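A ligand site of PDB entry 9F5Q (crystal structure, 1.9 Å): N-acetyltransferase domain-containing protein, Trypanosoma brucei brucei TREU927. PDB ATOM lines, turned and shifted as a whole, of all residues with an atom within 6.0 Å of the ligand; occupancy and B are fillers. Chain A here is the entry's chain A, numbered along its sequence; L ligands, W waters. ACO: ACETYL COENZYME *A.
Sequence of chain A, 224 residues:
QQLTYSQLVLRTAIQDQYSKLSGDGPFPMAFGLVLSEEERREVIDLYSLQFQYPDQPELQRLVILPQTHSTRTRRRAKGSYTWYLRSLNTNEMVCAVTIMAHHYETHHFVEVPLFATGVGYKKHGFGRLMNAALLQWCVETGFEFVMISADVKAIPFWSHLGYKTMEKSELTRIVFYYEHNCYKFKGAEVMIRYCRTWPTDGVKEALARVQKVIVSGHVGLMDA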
ATOM      1  N   LEU A   8      14.629 -13.716 -21.945  1.00  0.00           N
ATOM      2  CA  LEU A   8      15.467 -14.432 -21.001  1.00  0.00           C
ATOM      3  C   LEU A   8      16.920 -14.082 -21.229  1.00  0.00           C
ATOM      4  O   LEU A   8      17.493 -14.377 -22.278  1.00  0.00           O
ATOM      5  CB  LEU A   8      15.285 -15.946 -21.079  1.00  0.00           C
ATOM      6  CG  LEU A   8      16.172 -16.761 -20.137  1.00  0.00           C
ATOM      7  CD1 LEU A   8      15.966 -16.296 -18.699  1.00  0.00           C
ATOM      8  CD2 LEU A   8      15.967 -18.281 -20.288  1.00  0.00           C
ATOM      9  N   LEU A  10      20.266 -14.792 -19.004  1.00  0.00           N
ATOM     10  CA  LEU A  10      20.754 -15.484 -17.812  1.00  0.00           C
ATOM     11  C   LEU A  10      21.963 -14.724 -17.286  1.00  0.00           C
ATOM     12  O   LEU A  10      22.730 -14.172 -18.062  1.00  0.00           O
ATOM     13  CB  LEU A  10      21.088 -16.962 -18.055  1.00  0.00           C
ATOM     14  CG  LEU A  10      19.938 -17.913 -18.368  1.00  0.00           C
ATOM     15  CD1 LEU A  10      20.517 -19.152 -19.027  1.00  0.00           C
ATOM     16  CD2 LEU A  10      19.151 -18.319 -17.149  1.00  0.00           C
ATOM     17  N   GLN A  50      20.029 -15.653 -10.760  1.00  0.00           N
ATOM     18  CA  GLN A  50      19.921 -16.532 -11.926  1.00  0.00           C
ATOM     19  C   GLN A  50      19.661 -15.767 -13.221  1.00  0.00           C
ATOM     20  O   GLN A  50      20.181 -16.159 -14.287  1.00  0.00           O
ATOM     21  CB  GLN A  50      18.825 -17.584 -11.801  1.00  0.00           C
ATOM     22  CG  GLN A  50      18.958 -18.503 -10.613  1.00  0.00           C
ATOM     23  CD  GLN A  50      20.340 -19.083 -10.543  1.00  0.00           C
ATOM     24  OE1 GLN A  50      20.931 -19.496 -11.554  1.00  0.00           O
ATOM     25  NE2 GLN A  50      20.883 -19.111  -9.349  1.00  0.00           N
ATOM     26  N   PHE A  51      18.932 -14.643 -13.112  1.00  0.00           N
ATOM     27  CA  PHE A  51      18.533 -13.848 -14.255  1.00  0.00           C
ATOM     28  C   PHE A  51      19.149 -12.460 -14.226  1.00  0.00           C
ATOM     29  O   PHE A  51      19.125 -11.752 -13.195  1.00  0.00           O
ATOM     30  CB  PHE A  51      17.003 -13.710 -14.289  1.00  0.00           C
ATOM     31  CG  PHE A  51      16.221 -14.999 -14.113  1.00  0.00           C
ATOM     32  CD1 PHE A  51      16.220 -15.983 -15.100  1.00  0.00           C
ATOM     33  CD2 PHE A  51      15.519 -15.240 -12.925  1.00  0.00           C
ATOM     34  CE1 PHE A  51      15.455 -17.127 -14.954  1.00  0.00           C
ATOM     35  CE2 PHE A  51      14.820 -16.421 -12.752  1.00  0.00           C
ATOM     36  CZ  PHE A  51      14.803 -17.365 -13.754  1.00  0.00           C
ATOM     37  N   PRO A  54      14.454 -11.340 -16.672  1.00  0.00           N
ATOM     38  CA  PRO A  54      14.013 -10.209 -15.837  1.00  0.00           C
ATOM     39  C   PRO A  54      15.024  -9.551 -14.892  1.00  0.00           C
ATOM     40  O   PRO A  54      15.757 -10.205 -14.171  1.00  0.00           O
ATOM     41  CB  PRO A  54      12.843 -10.852 -15.042  1.00  0.00           C
ATOM     42  CG  PRO A  54      12.252 -11.847 -16.027  1.00  0.00           C
ATOM     43  CD  PRO A  54      13.469 -12.414 -16.743  1.00  0.00           C
ATOM     44  N   CYS A  95      14.576 -23.450  -4.121  1.00  0.00           N
ATOM     45  CA  CYS A  95      13.883 -23.516  -5.403  1.00  0.00           C
ATOM     46  C   CYS A  95      12.613 -22.673  -5.291  1.00  0.00           C
ATOM     47  O   CYS A  95      12.019 -22.567  -4.198  1.00  0.00           O
ATOM     48  CB  CYS A  95      13.471 -24.948  -5.728  1.00  0.00           C
ATOM     49  SG  CYS A  95      12.817 -25.112  -7.410  1.00  0.00           S
ATOM     50  N   VAL A 112       3.839 -20.343 -16.321  1.00  0.00           N
ATOM     51  CA  VAL A 112       4.954 -20.263 -15.381  1.00  0.00           C
ATOM     52  C   VAL A 112       5.994 -19.260 -15.865  1.00  0.00           C
ATOM     53  O   VAL A 112       6.891 -19.612 -16.625  1.00  0.00           O
ATOM     54  CB  VAL A 112       5.528 -21.679 -15.187  1.00  0.00           C
ATOM     55  CG1 VAL A 112       6.563 -21.745 -14.073  1.00  0.00           C
ATOM     56  CG2 VAL A 112       4.414 -22.694 -14.914  1.00  0.00           C
ATOM     57  N   PRO A 113       5.936 -17.973 -15.455  1.00  0.00           N
ATOM     58  CA  PRO A 113       6.932 -16.990 -15.843  1.00  0.00           C
ATOM     59  C   PRO A 113       8.354 -17.197 -15.314  1.00  0.00           C
ATOM     60  O   PRO A 113       9.305 -16.849 -16.022  1.00  0.00           O
ATOM     61  CB  PRO A 113       6.368 -15.666 -15.312  1.00  0.00           C
ATOM     62  CG  PRO A 113       4.890 -15.931 -15.222  1.00  0.00           C
ATOM     63  CD  PRO A 113       4.758 -17.365 -14.814  1.00  0.00           C
ATOM     64  N   LEU A 114       8.511 -17.709 -14.073  1.00  0.00           N
ATOM     65  CA  LEU A 114       9.830 -17.839 -13.447  1.00  0.00           C
ATOM     66  C   LEU A 114       9.928 -19.165 -12.710  1.00  0.00           C
ATOM     67  O   LEU A 114       9.023 -19.555 -11.976  1.00  0.00           O
ATOM     68  CB  LEU A 114      10.142 -16.714 -12.452  1.00  0.00           C
ATOM     69  CG  LEU A 114       9.951 -15.267 -12.928  1.00  0.00           C
ATOM     70  CD1 LEU A 114       9.841 -14.376 -11.729  1.00  0.00           C
ATOM     71  CD2 LEU A 114      11.059 -14.796 -13.838  1.00  0.00           C
ATOM     72  N   PHE A 115      11.099 -19.771 -12.756  1.00  0.00           N
ATOM     73  CA  PHE A 115      11.370 -21.018 -12.070  1.00  0.00           C
ATOM     74  C   PHE A 115      12.877 -21.085 -11.898  1.00  0.00           C
ATOM     75  O   PHE A 115      13.588 -20.995 -12.856  1.00  0.00           O
ATOM     76  CB  PHE A 115      10.809 -22.197 -12.886  1.00  0.00           C
ATOM     77  CG  PHE A 115      10.880 -23.573 -12.208  1.00  0.00           C
ATOM     78  CD1 PHE A 115      12.106 -24.181 -11.901  1.00  0.00           C
ATOM     79  CD2 PHE A 115       9.730 -24.271 -11.936  1.00  0.00           C
ATOM     80  CE1 PHE A 115      12.143 -25.413 -11.263  1.00  0.00           C
ATOM     81  CE2 PHE A 115       9.771 -25.510 -11.319  1.00  0.00           C
ATOM     82  CZ  PHE A 115      10.966 -26.072 -10.980  1.00  0.00           C
ATOM     83  N   ALA A 116      13.363 -21.208 -10.665  1.00  0.00           N
ATOM     84  CA  ALA A 116      14.802 -21.251 -10.477  1.00  0.00           C
ATOM     85  C   ALA A 116      15.146 -22.111  -9.266  1.00  0.00           C
ATOM     86  O   ALA A 116      14.374 -22.154  -8.285  1.00  0.00           O
ATOM     87  CB  ALA A 116      15.355 -19.856 -10.310  1.00  0.00           C
ATOM     88  N   THR A 117      16.318 -22.754  -9.361  1.00  0.00           N
ATOM     89  CA  THR A 117      16.946 -23.452  -8.243  1.00  0.00           C
ATOM     90  C   THR A 117      18.217 -22.699  -7.839  1.00  0.00           C
ATOM     91  O   THR A 117      19.003 -22.276  -8.696  1.00  0.00           O
ATOM     92  CB  THR A 117      17.227 -24.894  -8.667  1.00  0.00           C
ATOM     93  OG1 THR A 117      15.956 -25.535  -8.662  1.00  0.00           O
ATOM     94  CG2 THR A 117      18.159 -25.622  -7.716  1.00  0.00           C
ATOM     95  N   GLY A 118      18.438 -22.521  -6.518  1.00  0.00           N
ATOM     96  CA  GLY A 118      19.538 -21.709  -6.015  1.00  0.00           C
ATOM     97  C   GLY A 118      20.926 -22.318  -6.220  1.00  0.00           C
ATOM     98  O   GLY A 118      21.088 -23.504  -6.502  1.00  0.00           O
ATOM     99  N   TYR A 121      22.481 -25.919  -5.106  1.00  0.00           N
ATOM    100  CA  TYR A 121      21.355 -26.841  -5.021  1.00  0.00           C
ATOM    101  C   TYR A 121      20.943 -27.426  -6.365  1.00  0.00           C
ATOM    102  O   TYR A 121      20.037 -28.270  -6.405  1.00  0.00           O
ATOM    103  CB  TYR A 121      20.083 -26.174  -4.480  1.00  0.00           C
ATOM    104  CG  TYR A 121      20.248 -25.666  -3.063  1.00  0.00           C
ATOM    105  CD1 TYR A 121      20.291 -26.540  -2.003  1.00  0.00           C
ATOM    106  CD2 TYR A 121      20.300 -24.306  -2.801  1.00  0.00           C
ATOM    107  CE1 TYR A 121      20.402 -26.081  -0.696  1.00  0.00           C
ATOM    108  CE2 TYR A 121      20.432 -23.843  -1.506  1.00  0.00           C
ATOM    109  CZ  TYR A 121      20.487 -24.729  -0.446  1.00  0.00           C
ATOM    110  OH  TYR A 121      20.608 -24.268   0.863  1.00  0.00           O
ATOM    111  N   LYS A 122      21.611 -26.987  -7.446  1.00  0.00           N
ATOM    112  CA  LYS A 122      21.291 -27.399  -8.785  1.00  0.00           C
ATOM    113  C   LYS A 122      21.673 -28.868  -9.010  1.00  0.00           C
ATOM    114  O   LYS A 122      22.626 -29.373  -8.457  1.00  0.00           O
ATOM    115  CB  LYS A 122      21.943 -26.487  -9.831  1.00  0.00           C
ATOM    116  CG  LYS A 122      21.351 -25.078  -9.906  1.00  0.00           C
ATOM    117  CD  LYS A 122      21.994 -24.213 -10.981  1.00  0.00           C
ATOM    118  CE  LYS A 122      21.410 -22.839 -11.090  1.00  0.00           C
ATOM    119  NZ  LYS A 122      21.623 -22.498 -12.511  1.00  0.00           N
ATOM    120  N   LYS A 123      20.899 -29.524  -9.865  1.00  0.00           N
ATOM    121  CA  LYS A 123      21.174 -30.861 -10.327  1.00  0.00           C
ATOM    122  C   LYS A 123      21.143 -31.875  -9.172  1.00  0.00           C
ATOM    123  O   LYS A 123      21.893 -32.858  -9.232  1.00  0.00           O
ATOM    124  CB  LYS A 123      22.476 -30.899 -11.129  1.00  0.00           C
ATOM    125  CG  LYS A 123      22.387 -30.155 -12.460  1.00  0.00           C
ATOM    126  CD  LYS A 123      23.655 -30.272 -13.306  1.00  0.00           C
ATOM    127  CE  LYS A 123      23.498 -29.751 -14.703  1.00  0.00           C
ATOM    128  NZ  LYS A 123      24.771 -29.445 -15.385  1.00  0.00           N
ATOM    129  N   HIS A 124      20.291 -31.601  -8.160  1.00  0.00           N
ATOM    130  CA  HIS A 124      19.996 -32.534  -7.070  1.00  0.00           C
ATOM    131  C   HIS A 124      18.551 -33.079  -7.151  1.00  0.00           C
ATOM    132  O   HIS A 124      18.116 -33.864  -6.309  1.00  0.00           O
ATOM    133  CB  HIS A 124      20.120 -31.834  -5.701  1.00  0.00           C
ATOM    134  CG  HIS A 124      21.518 -31.453  -5.303  1.00  0.00           C
ATOM    135  ND1 HIS A 124      22.306 -30.588  -6.018  1.00  0.00           N
ATOM    136  CD2 HIS A 124      22.224 -31.785  -4.191  1.00  0.00           C
ATOM    137  CE1 HIS A 124      23.483 -30.485  -5.406  1.00  0.00           C
ATOM    138  NE2 HIS A 124      23.461 -31.196  -4.284  1.00  0.00           N
ATOM    139  N   GLY A 125      17.769 -32.613  -8.129  1.00  0.00           N
ATOM    140  CA  GLY A 125      16.395 -33.068  -8.269  1.00  0.00           C
ATOM    141  C   GLY A 125      15.366 -32.146  -7.649  1.00  0.00           C
ATOM    142  O   GLY A 125      14.162 -32.474  -7.656  1.00  0.00           O
ATOM    143  N   PHE A 126      15.783 -30.941  -7.264  1.00  0.00           N
ATOM    144  CA  PHE A 126      14.836 -30.020  -6.637  1.00  0.00           C
ATOM    145  C   PHE A 126      13.873 -29.429  -7.660  1.00  0.00           C
ATOM    146  O   PHE A 126      12.703 -29.225  -7.360  1.00  0.00           O
ATOM    147  CB  PHE A 126      15.543 -28.883  -5.901  1.00  0.00           C
ATOM    148  CG  PHE A 126      16.209 -29.340  -4.641  1.00  0.00           C
ATOM    149  CD1 PHE A 126      15.448 -29.730  -3.534  1.00  0.00           C
ATOM    150  CD2 PHE A 126      17.589 -29.403  -4.564  1.00  0.00           C
ATOM    151  CE1 PHE A 126      16.069 -30.125  -2.364  1.00  0.00           C
ATOM    152  CE2 PHE A 126      18.197 -29.786  -3.382  1.00  0.00           C
ATOM    153  CZ  PHE A 126      17.454 -30.152  -2.294  1.00  0.00           C
ATOM    154  N   GLY A 127      14.357 -29.098  -8.867  1.00  0.00           N
ATOM    155  CA  GLY A 127      13.470 -28.638  -9.910  1.00  0.00           C
ATOM    156  C   GLY A 127      12.346 -29.635 -10.200  1.00  0.00           C
ATOM    157  O   GLY A 127      11.182 -29.240 -10.285  1.00  0.00           O
ATOM    158  N   ARG A 128      12.699 -30.914 -10.365  1.00  0.00           N
ATOM    159  CA  ARG A 128      11.713 -31.957 -10.615  1.00  0.00           C
ATOM    160  C   ARG A 128      10.688 -32.012  -9.498  1.00  0.00           C
ATOM    161  O   ARG A 128       9.484 -32.066  -9.743  1.00  0.00           O
ATOM    162  CB  ARG A 128      12.415 -33.303 -10.780  1.00  0.00           C
ATOM    163  CG  ARG A 128      11.500 -34.453 -11.177  1.00  0.00           C
ATOM    164  CD  ARG A 128      12.198 -35.771 -11.095  1.00  0.00           C
ATOM    165  NE  ARG A 128      13.362 -35.857 -11.972  1.00  0.00           N
ATOM    166  CZ  ARG A 128      14.628 -36.002 -11.548  1.00  0.00           C
ATOM    167  NH1 ARG A 128      14.992 -36.037 -10.262  1.00  0.00           N
ATOM    168  NH2 ARG A 128      15.585 -36.117 -12.448  1.00  0.00           N
ATOM    169  N   LEU A 129      11.182 -31.954  -8.259  1.00  0.00           N
ATOM    170  CA  LEU A 129      10.337 -31.961  -7.072  1.00  0.00           C
ATOM    171  C   LEU A 129       9.406 -30.746  -7.065  1.00  0.00           C
ATOM    172  O   LEU A 129       8.233 -30.927  -6.895  1.00  0.00           O
ATOM    173  CB  LEU A 129      11.189 -31.983  -5.804  1.00  0.00           C
ATOM    174  CG  LEU A 129      10.403 -31.868  -4.492  1.00  0.00           C
ATOM    175  CD1 LEU A 129       9.319 -32.962  -4.408  1.00  0.00           C
ATOM    176  CD2 LEU A 129      11.320 -31.938  -3.289  1.00  0.00           C
ATOM    177  N   LYS A 153      16.985 -21.509 -24.373  1.00  0.00           N
ATOM    178  CA  LYS A 153      17.861 -22.065 -23.351  1.00  0.00           C
ATOM    179  C   LYS A 153      17.104 -22.858 -22.293  1.00  0.00           C
ATOM    180  O   LYS A 153      17.740 -23.689 -21.620  1.00  0.00           O
ATOM    181  CB  LYS A 153      18.692 -20.965 -22.689  1.00  0.00           C
ATOM    182  CG  LYS A 153      19.834 -20.429 -23.527  1.00  0.00           C
ATOM    183  CD  LYS A 153      20.806 -19.636 -22.658  1.00  0.00           C
ATOM    184  CE  LYS A 153      21.900 -19.021 -23.458  1.00  0.00           C
ATOM    185  NZ  LYS A 153      21.397 -18.060 -24.435  1.00  0.00           N
ATOM    186  N   ALA A 154      15.787 -22.582 -22.106  1.00  0.00           N
ATOM    187  CA  ALA A 154      14.940 -23.285 -21.135  1.00  0.00           C
ATOM    188  C   ALA A 154      14.339 -24.585 -21.676  1.00  0.00           C
ATOM    189  O   ALA A 154      13.935 -25.467 -20.887  1.00  0.00           O
ATOM    190  CB  ALA A 154      13.848 -22.343 -20.656  1.00  0.00           C
ATOM    191  N   PRO A 156      15.378 -27.438 -23.105  1.00  0.00           N
ATOM    192  CA  PRO A 156      15.833 -28.753 -22.666  1.00  0.00           C
ATOM    193  C   PRO A 156      15.335 -29.037 -21.247  1.00  0.00           C
ATOM    194  O   PRO A 156      14.846 -30.121 -20.988  1.00  0.00           O
ATOM    195  CB  PRO A 156      17.336 -28.634 -22.745  1.00  0.00           C
ATOM    196  CG  PRO A 156      17.641 -27.398 -23.603  1.00  0.00           C
ATOM    197  CD  PRO A 156      16.449 -26.521 -23.521  1.00  0.00           C
ATOM    198  N   PHE A 157      15.437 -28.073 -20.331  1.00  0.00           N
ATOM    199  CA  PHE A 157      14.939 -28.266 -18.992  1.00  0.00           C
ATOM    200  C   PHE A 157      13.465 -28.671 -19.020  1.00  0.00           C
ATOM    201  O   PHE A 157      13.065 -29.709 -18.434  1.00  0.00           O
ATOM    202  CB  PHE A 157      15.220 -27.015 -18.150  1.00  0.00           C
ATOM    203  CG  PHE A 157      14.428 -26.973 -16.838  1.00  0.00           C
ATOM    204  CD1 PHE A 157      14.615 -27.932 -15.873  1.00  0.00           C
ATOM    205  CD2 PHE A 157      13.453 -26.011 -16.612  1.00  0.00           C
ATOM    206  CE1 PHE A 157      13.906 -27.901 -14.689  1.00  0.00           C
ATOM    207  CE2 PHE A 157      12.745 -25.994 -15.413  1.00  0.00           C
ATOM    208  CZ  PHE A 157      13.005 -26.904 -14.436  1.00  0.00           C
ATOM    209  N   TRP A 158      12.609 -27.834 -19.626  1.00  0.00           N
ATOM    210  CA  TRP A 158      11.182 -28.097 -19.539  1.00  0.00           C
ATOM    211  C   TRP A 158      10.852 -29.452 -20.171  1.00  0.00           C
ATOM    212  O   TRP A 158      10.047 -30.241 -19.671  1.00  0.00           O
ATOM    213  CB  TRP A 158      10.380 -26.978 -20.174  1.00  0.00           C
ATOM    214  CG  TRP A 158      10.467 -25.691 -19.405  1.00  0.00           C
ATOM    215  CD1 TRP A 158      10.990 -24.505 -19.820  1.00  0.00           C
ATOM    216  CD2 TRP A 158       9.978 -25.474 -18.078  1.00  0.00           C
ATOM    217  NE1 TRP A 158      10.858 -23.573 -18.829  1.00  0.00           N
ATOM    218  CE2 TRP A 158      10.220 -24.122 -17.759  1.00  0.00           C
ATOM    219  CE3 TRP A 158       9.344 -26.277 -17.139  1.00  0.00           C
ATOM    220  CZ2 TRP A 158       9.872 -23.573 -16.518  1.00  0.00           C
ATOM    221  CZ3 TRP A 158       8.987 -25.723 -15.920  1.00  0.00           C
ATOM    222  CH2 TRP A 158       9.226 -24.394 -15.622  1.00  0.00           C
ATOM    223  N   HIS A 160      12.827 -32.074 -20.278  1.00  0.00           N
ATOM    224  CA  HIS A 160      13.151 -33.110 -19.329  1.00  0.00           C
ATOM    225  C   HIS A 160      12.102 -33.249 -18.234  1.00  0.00           C
ATOM    226  O   HIS A 160      12.034 -34.278 -17.614  1.00  0.00           O
ATOM    227  CB  HIS A 160      14.527 -32.884 -18.675  1.00  0.00           C
ATOM    228  CG  HIS A 160      15.703 -33.353 -19.474  1.00  0.00           C
ATOM    229  ND1 HIS A 160      16.214 -34.624 -19.329  1.00  0.00           N
ATOM    230  CD2 HIS A 160      16.505 -32.734 -20.340  1.00  0.00           C
ATOM    231  CE1 HIS A 160      17.244 -34.782 -20.152  1.00  0.00           C
ATOM    232  NE2 HIS A 160      17.446 -33.650 -20.769  1.00  0.00           N
ATOM    233  N   LEU A 161      11.337 -32.176 -17.935  1.00  0.00           N
ATOM    234  CA  LEU A 161      10.331 -32.251 -16.880  1.00  0.00           C
ATOM    235  C   LEU A 161       9.038 -32.805 -17.452  1.00  0.00           C
ATOM    236  O   LEU A 161       8.032 -32.904 -16.738  1.00  0.00           O
ATOM    237  CB  LEU A 161      10.058 -30.901 -16.213  1.00  0.00           C
ATOM    238  CG  LEU A 161      11.126 -30.334 -15.276  1.00  0.00           C
ATOM    239  CD1 LEU A 161      10.590 -29.031 -14.657  1.00  0.00           C
ATOM    240  CD2 LEU A 161      11.524 -31.311 -14.222  1.00  0.00           C
ATOM    241  N   PHE A 185       8.189 -14.882 -23.704  1.00  0.00           N
ATOM    242  CA  PHE A 185       9.608 -14.650 -23.876  1.00  0.00           C
ATOM    243  C   PHE A 185       9.876 -14.531 -25.361  1.00  0.00           C
ATOM    244  O   PHE A 185       9.345 -15.322 -26.144  1.00  0.00           O
ATOM    245  CB  PHE A 185      10.439 -15.764 -23.226  1.00  0.00           C
ATOM    246  CG  PHE A 185      10.447 -15.676 -21.708  1.00  0.00           C
ATOM    247  CD1 PHE A 185      11.334 -14.832 -21.045  1.00  0.00           C
ATOM    248  CD2 PHE A 185       9.575 -16.433 -20.952  1.00  0.00           C
ATOM    249  CE1 PHE A 185      11.324 -14.758 -19.650  1.00  0.00           C
ATOM    250  CE2 PHE A 185       9.552 -16.340 -19.564  1.00  0.00           C
ATOM    251  CZ  PHE A 185      10.413 -15.508 -18.925  1.00  0.00           C
ATOM    252  N   ARG A 209      13.766 -39.089  -5.202  1.00  0.00           N
ATOM    253  CA  ARG A 209      14.982 -38.926  -6.000  1.00  0.00           C
ATOM    254  C   ARG A 209      15.847 -37.775  -5.499  1.00  0.00           C
ATOM    255  O   ARG A 209      16.911 -37.567  -6.034  1.00  0.00           O
ATOM    256  CB  ARG A 209      14.682 -38.814  -7.508  1.00  0.00           C
ATOM    257  CG  ARG A 209      13.956 -40.043  -8.053  1.00  0.00           C
ATOM    258  CD  ARG A 209      13.683 -40.019  -9.565  1.00  0.00           C
ATOM    259  NE  ARG A 209      14.943 -40.070 -10.321  1.00  0.00           N
ATOM    260  CZ  ARG A 209      15.152 -39.761 -11.607  1.00  0.00           C
ATOM    261  NH1 ARG A 209      14.159 -39.348 -12.368  1.00  0.00           N
ATOM    262  NH2 ARG A 209      16.382 -39.817 -12.103  1.00  0.00           N
HETATM  263  N1A ACO L   1      19.602 -28.065 -18.880  1.00  0.00           N
HETATM  264  C2A ACO L   1      18.780 -29.062 -19.252  1.00  0.00           C
HETATM  265  N3A ACO L   1      18.195 -29.991 -18.505  1.00  0.00           N
HETATM  266  C4A ACO L   1      18.545 -29.835 -17.216  1.00  0.00           C
HETATM  267  C5A ACO L   1      19.360 -28.871 -16.682  1.00  0.00           C
HETATM  268  C6A ACO L   1      19.914 -27.937 -17.573  1.00  0.00           C
HETATM  269  N6A ACO L   1      20.741 -26.962 -17.208  1.00  0.00           N
HETATM  270  N7A ACO L   1      19.476 -29.041 -15.308  1.00  0.00           N
HETATM  271  C8A ACO L   1      18.725 -30.085 -15.041  1.00  0.00           C
HETATM  272  N9A ACO L   1      18.151 -30.606 -16.158  1.00  0.00           N
HETATM  273  C1B ACO L   1      17.258 -31.736 -16.221  1.00  0.00           C
HETATM  274  C2B ACO L   1      17.713 -32.895 -15.359  1.00  0.00           C
HETATM  275  O2B ACO L   1      18.610 -33.733 -16.055  1.00  0.00           O
HETATM  276  C3B ACO L   1      16.380 -33.559 -15.039  1.00  0.00           C
HETATM  277  O3B ACO L   1      15.940 -34.308 -16.163  1.00  0.00           O
HETATM  278  P3B ACO L   1      16.054 -35.891 -15.961  1.00  0.00           P
HETATM  279  O7A ACO L   1      15.038 -36.300 -14.930  1.00  0.00           O
HETATM  280  O8A ACO L   1      17.458 -36.184 -15.524  1.00  0.00           O
HETATM  281  O9A ACO L   1      15.764 -36.470 -17.310  1.00  0.00           O
HETATM  282  C4B ACO L   1      15.457 -32.352 -14.847  1.00  0.00           C
HETATM  283  O4B ACO L   1      16.021 -31.314 -15.696  1.00  0.00           O
HETATM  284  C5B ACO L   1      15.315 -31.833 -13.433  1.00  0.00           C
HETATM  285  O5B ACO L   1      16.613 -31.602 -12.849  1.00  0.00           O
HETATM  286  P1A ACO L   1      16.732 -30.893 -11.430  1.00  0.00           P
HETATM  287  O1A ACO L   1      18.003 -31.276 -10.776  1.00  0.00           O
HETATM  288  O2A ACO L   1      15.465 -31.088 -10.671  1.00  0.00           O
HETATM  289  O3A ACO L   1      16.828 -29.359 -11.863  1.00  0.00           O
HETATM  290  P2A ACO L   1      17.487 -28.156 -11.047  1.00  0.00           P
HETATM  291  O4A ACO L   1      16.976 -28.185  -9.662  1.00  0.00           O
HETATM  292  O5A ACO L   1      18.956 -28.184 -11.275  1.00  0.00           O
HETATM  293  O6A ACO L   1      16.846 -26.875 -11.777  1.00  0.00           O
HETATM  294  CBP ACO L   1      17.001 -25.135 -13.429  1.00  0.00           C
HETATM  295  CCP ACO L   1      17.127 -26.636 -13.177  1.00  0.00           C
HETATM  296  CDP ACO L   1      16.952 -24.886 -14.940  1.00  0.00           C
HETATM  297  CEP ACO L   1      15.717 -24.604 -12.809  1.00  0.00           C
HETATM  298  CAP ACO L   1      18.212 -24.423 -12.823  1.00  0.00           C
HETATM  299  OAP ACO L   1      19.365 -24.801 -13.547  1.00  0.00           O
HETATM  300  C9P ACO L   1      18.111 -22.903 -12.796  1.00  0.00           C
HETATM  301  O9P ACO L   1      17.688 -22.338 -11.796  1.00  0.00           O
HETATM  302  N8P ACO L   1      18.525 -22.243 -13.865  1.00  0.00           N
HETATM  303  C7P ACO L   1      18.519 -20.796 -13.958  1.00  0.00           C
HETATM  304  C6P ACO L   1      17.145 -20.241 -14.204  1.00  0.00           C
HETATM  305  C5P ACO L   1      16.467 -20.890 -15.392  1.00  0.00           C
HETATM  306  O5P ACO L   1      17.090 -21.126 -16.431  1.00  0.00           O
HETATM  307  N4P ACO L   1      15.176 -21.186 -15.265  1.00  0.00           N
HETATM  308  C3P ACO L   1      14.520 -22.277 -15.976  1.00  0.00           C
HETATM  309  C2P ACO L   1      13.359 -21.802 -16.815  1.00  0.00           C
HETATM  310  S1P ACO L   1      13.581 -20.137 -17.467  1.00  0.00           S
HETATM  311  C   ACO L   1      12.827 -18.893 -16.524  1.00  0.00           C
HETATM  312  O   ACO L   1      12.398 -19.087 -15.414  1.00  0.00           O
HETATM  313  CH3 ACO L   1      12.748 -17.583 -17.209  1.00  0.00           C
HETATM  314  O   HOH W   1      21.245 -33.274 -15.487  1.00  0.00           O
HETATM  315  O   HOH W   2      18.308 -29.559  -7.924  1.00  0.00           O
HETATM  316  O   HOH W   3      13.235 -36.852 -18.105  1.00  0.00           O
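Merely in contact with the ligand: Leu 8 (3.8 Å), Leu 10 (3.6 Å), Gln 50 (3.6 Å), Phe 51 (3.4 Å), Pro 113 (3.7 Å), Leu 114 (3.5 Å), Ala 116 (3.4 Å), Ala 154 (3.9 Å), Pro 156 (3.8 Å), Phe 157 (3.6 Å), Trp 158 (3.7 Å), Leu 161 (3.9 Å) and Phe 185 (3.6 Å). Hydrophobic or aromatic side chains within 4 Å of the ligand: Leu 8, Leu 10, Phe 51, Phe 115, Ala 116, Ala 154, Pro 156, Phe 157, Trp 158, His 160, Leu 161 and Phe 185. 23 residues have an atom within 4 Å of the ligand: Leu 8, Leu 10, Gln 50, Phe 51, Pro 113, Leu 114, Phe 115, Ala 116, Thr 117, Lys 122, Lys 123, His 124, Gly 125, Phe 126, Gly 127, Arg 128, Ala 154, Pro 156, Phe 157, Trp 158, His 160, Leu 161 and Phe 185. The nearest printed residue that does not touch the ligand is Arg 209 (4.1 Å).
NZ of Lys 122 is in hydrogen-bond range of OE1 of Gln 50 (3.2 Å). The side-chain sulfur (SG) of Cys 95 is in hydrogen-bond range of the side-chain hydroxyl (OG1) of Thr 117, 3.4 Å away. O of Ala 116 lies close to SG of Cys 95 (3.5 Å). The backbone carbonyl oxygen (O) of Lys 122 sits at hydrogen-bond distance from a ring nitrogen (ND1) of His 124 (2.7 Å). O of Tyr 121 lies within hydrogen-bond range of ND1 of His 124 (3.3 Å).
The backbone NH of Lys 123 lies within hydrogen-bond range of an oxygen (O5A) of the ligand. N of Arg 128 lies within hydrogen-bond range of O2A of the ligand (2.8 Å). N of Gly 127 sits at hydrogen-bond distance from O4A of the ligand (2.9 Å). An oxygen (O1A) of the ligand lies within hydrogen-bond range of the backbone NH (N) of Gly 125, at 3.0 Å. An oxygen (OAP) of the ligand is in hydrogen-bond range of the side-chain amino group (NZ) of Lys 122 (3.4 Å). The side-chain hydroxyl of Thr 117 sits at hydrogen-bond distance from an oxygen (O4A) of the ligand, 3.0 Å away. N of Phe 115 is in hydrogen-bond range of O of the ligand, 3.0 Å away. NH2 of Arg 128 is in salt-bridge range of O7A of the ligand (2.5 Å). N of Phe 126 is in hydrogen-bond range of O2A of the ligand, 3.4 Å away. The backbone NH (N) of Thr 117 lies within hydrogen-bond range of an oxygen (O9P) of the ligand, 2.8 Å away. The backbone carbonyl oxygen of Phe 115 sits at hydrogen-bond distance from a nitrogen (N4P) of the ligand (2.9 Å). An oxygen (O9A) of the ligand sits at hydrogen-bond distance from a ring nitrogen (ND1) of His 160, 2.8 Å away. The backbone NH (N) of His 124 sits at hydrogen-bond distance from an oxygen (O1A) of the ligand, 3.5 Å away.
Water W3 bridges an oxygen (O9A) of the ligand (2.7 Å) and the backbone carbonyl oxygen (O) of His 160 (2.9 Å).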
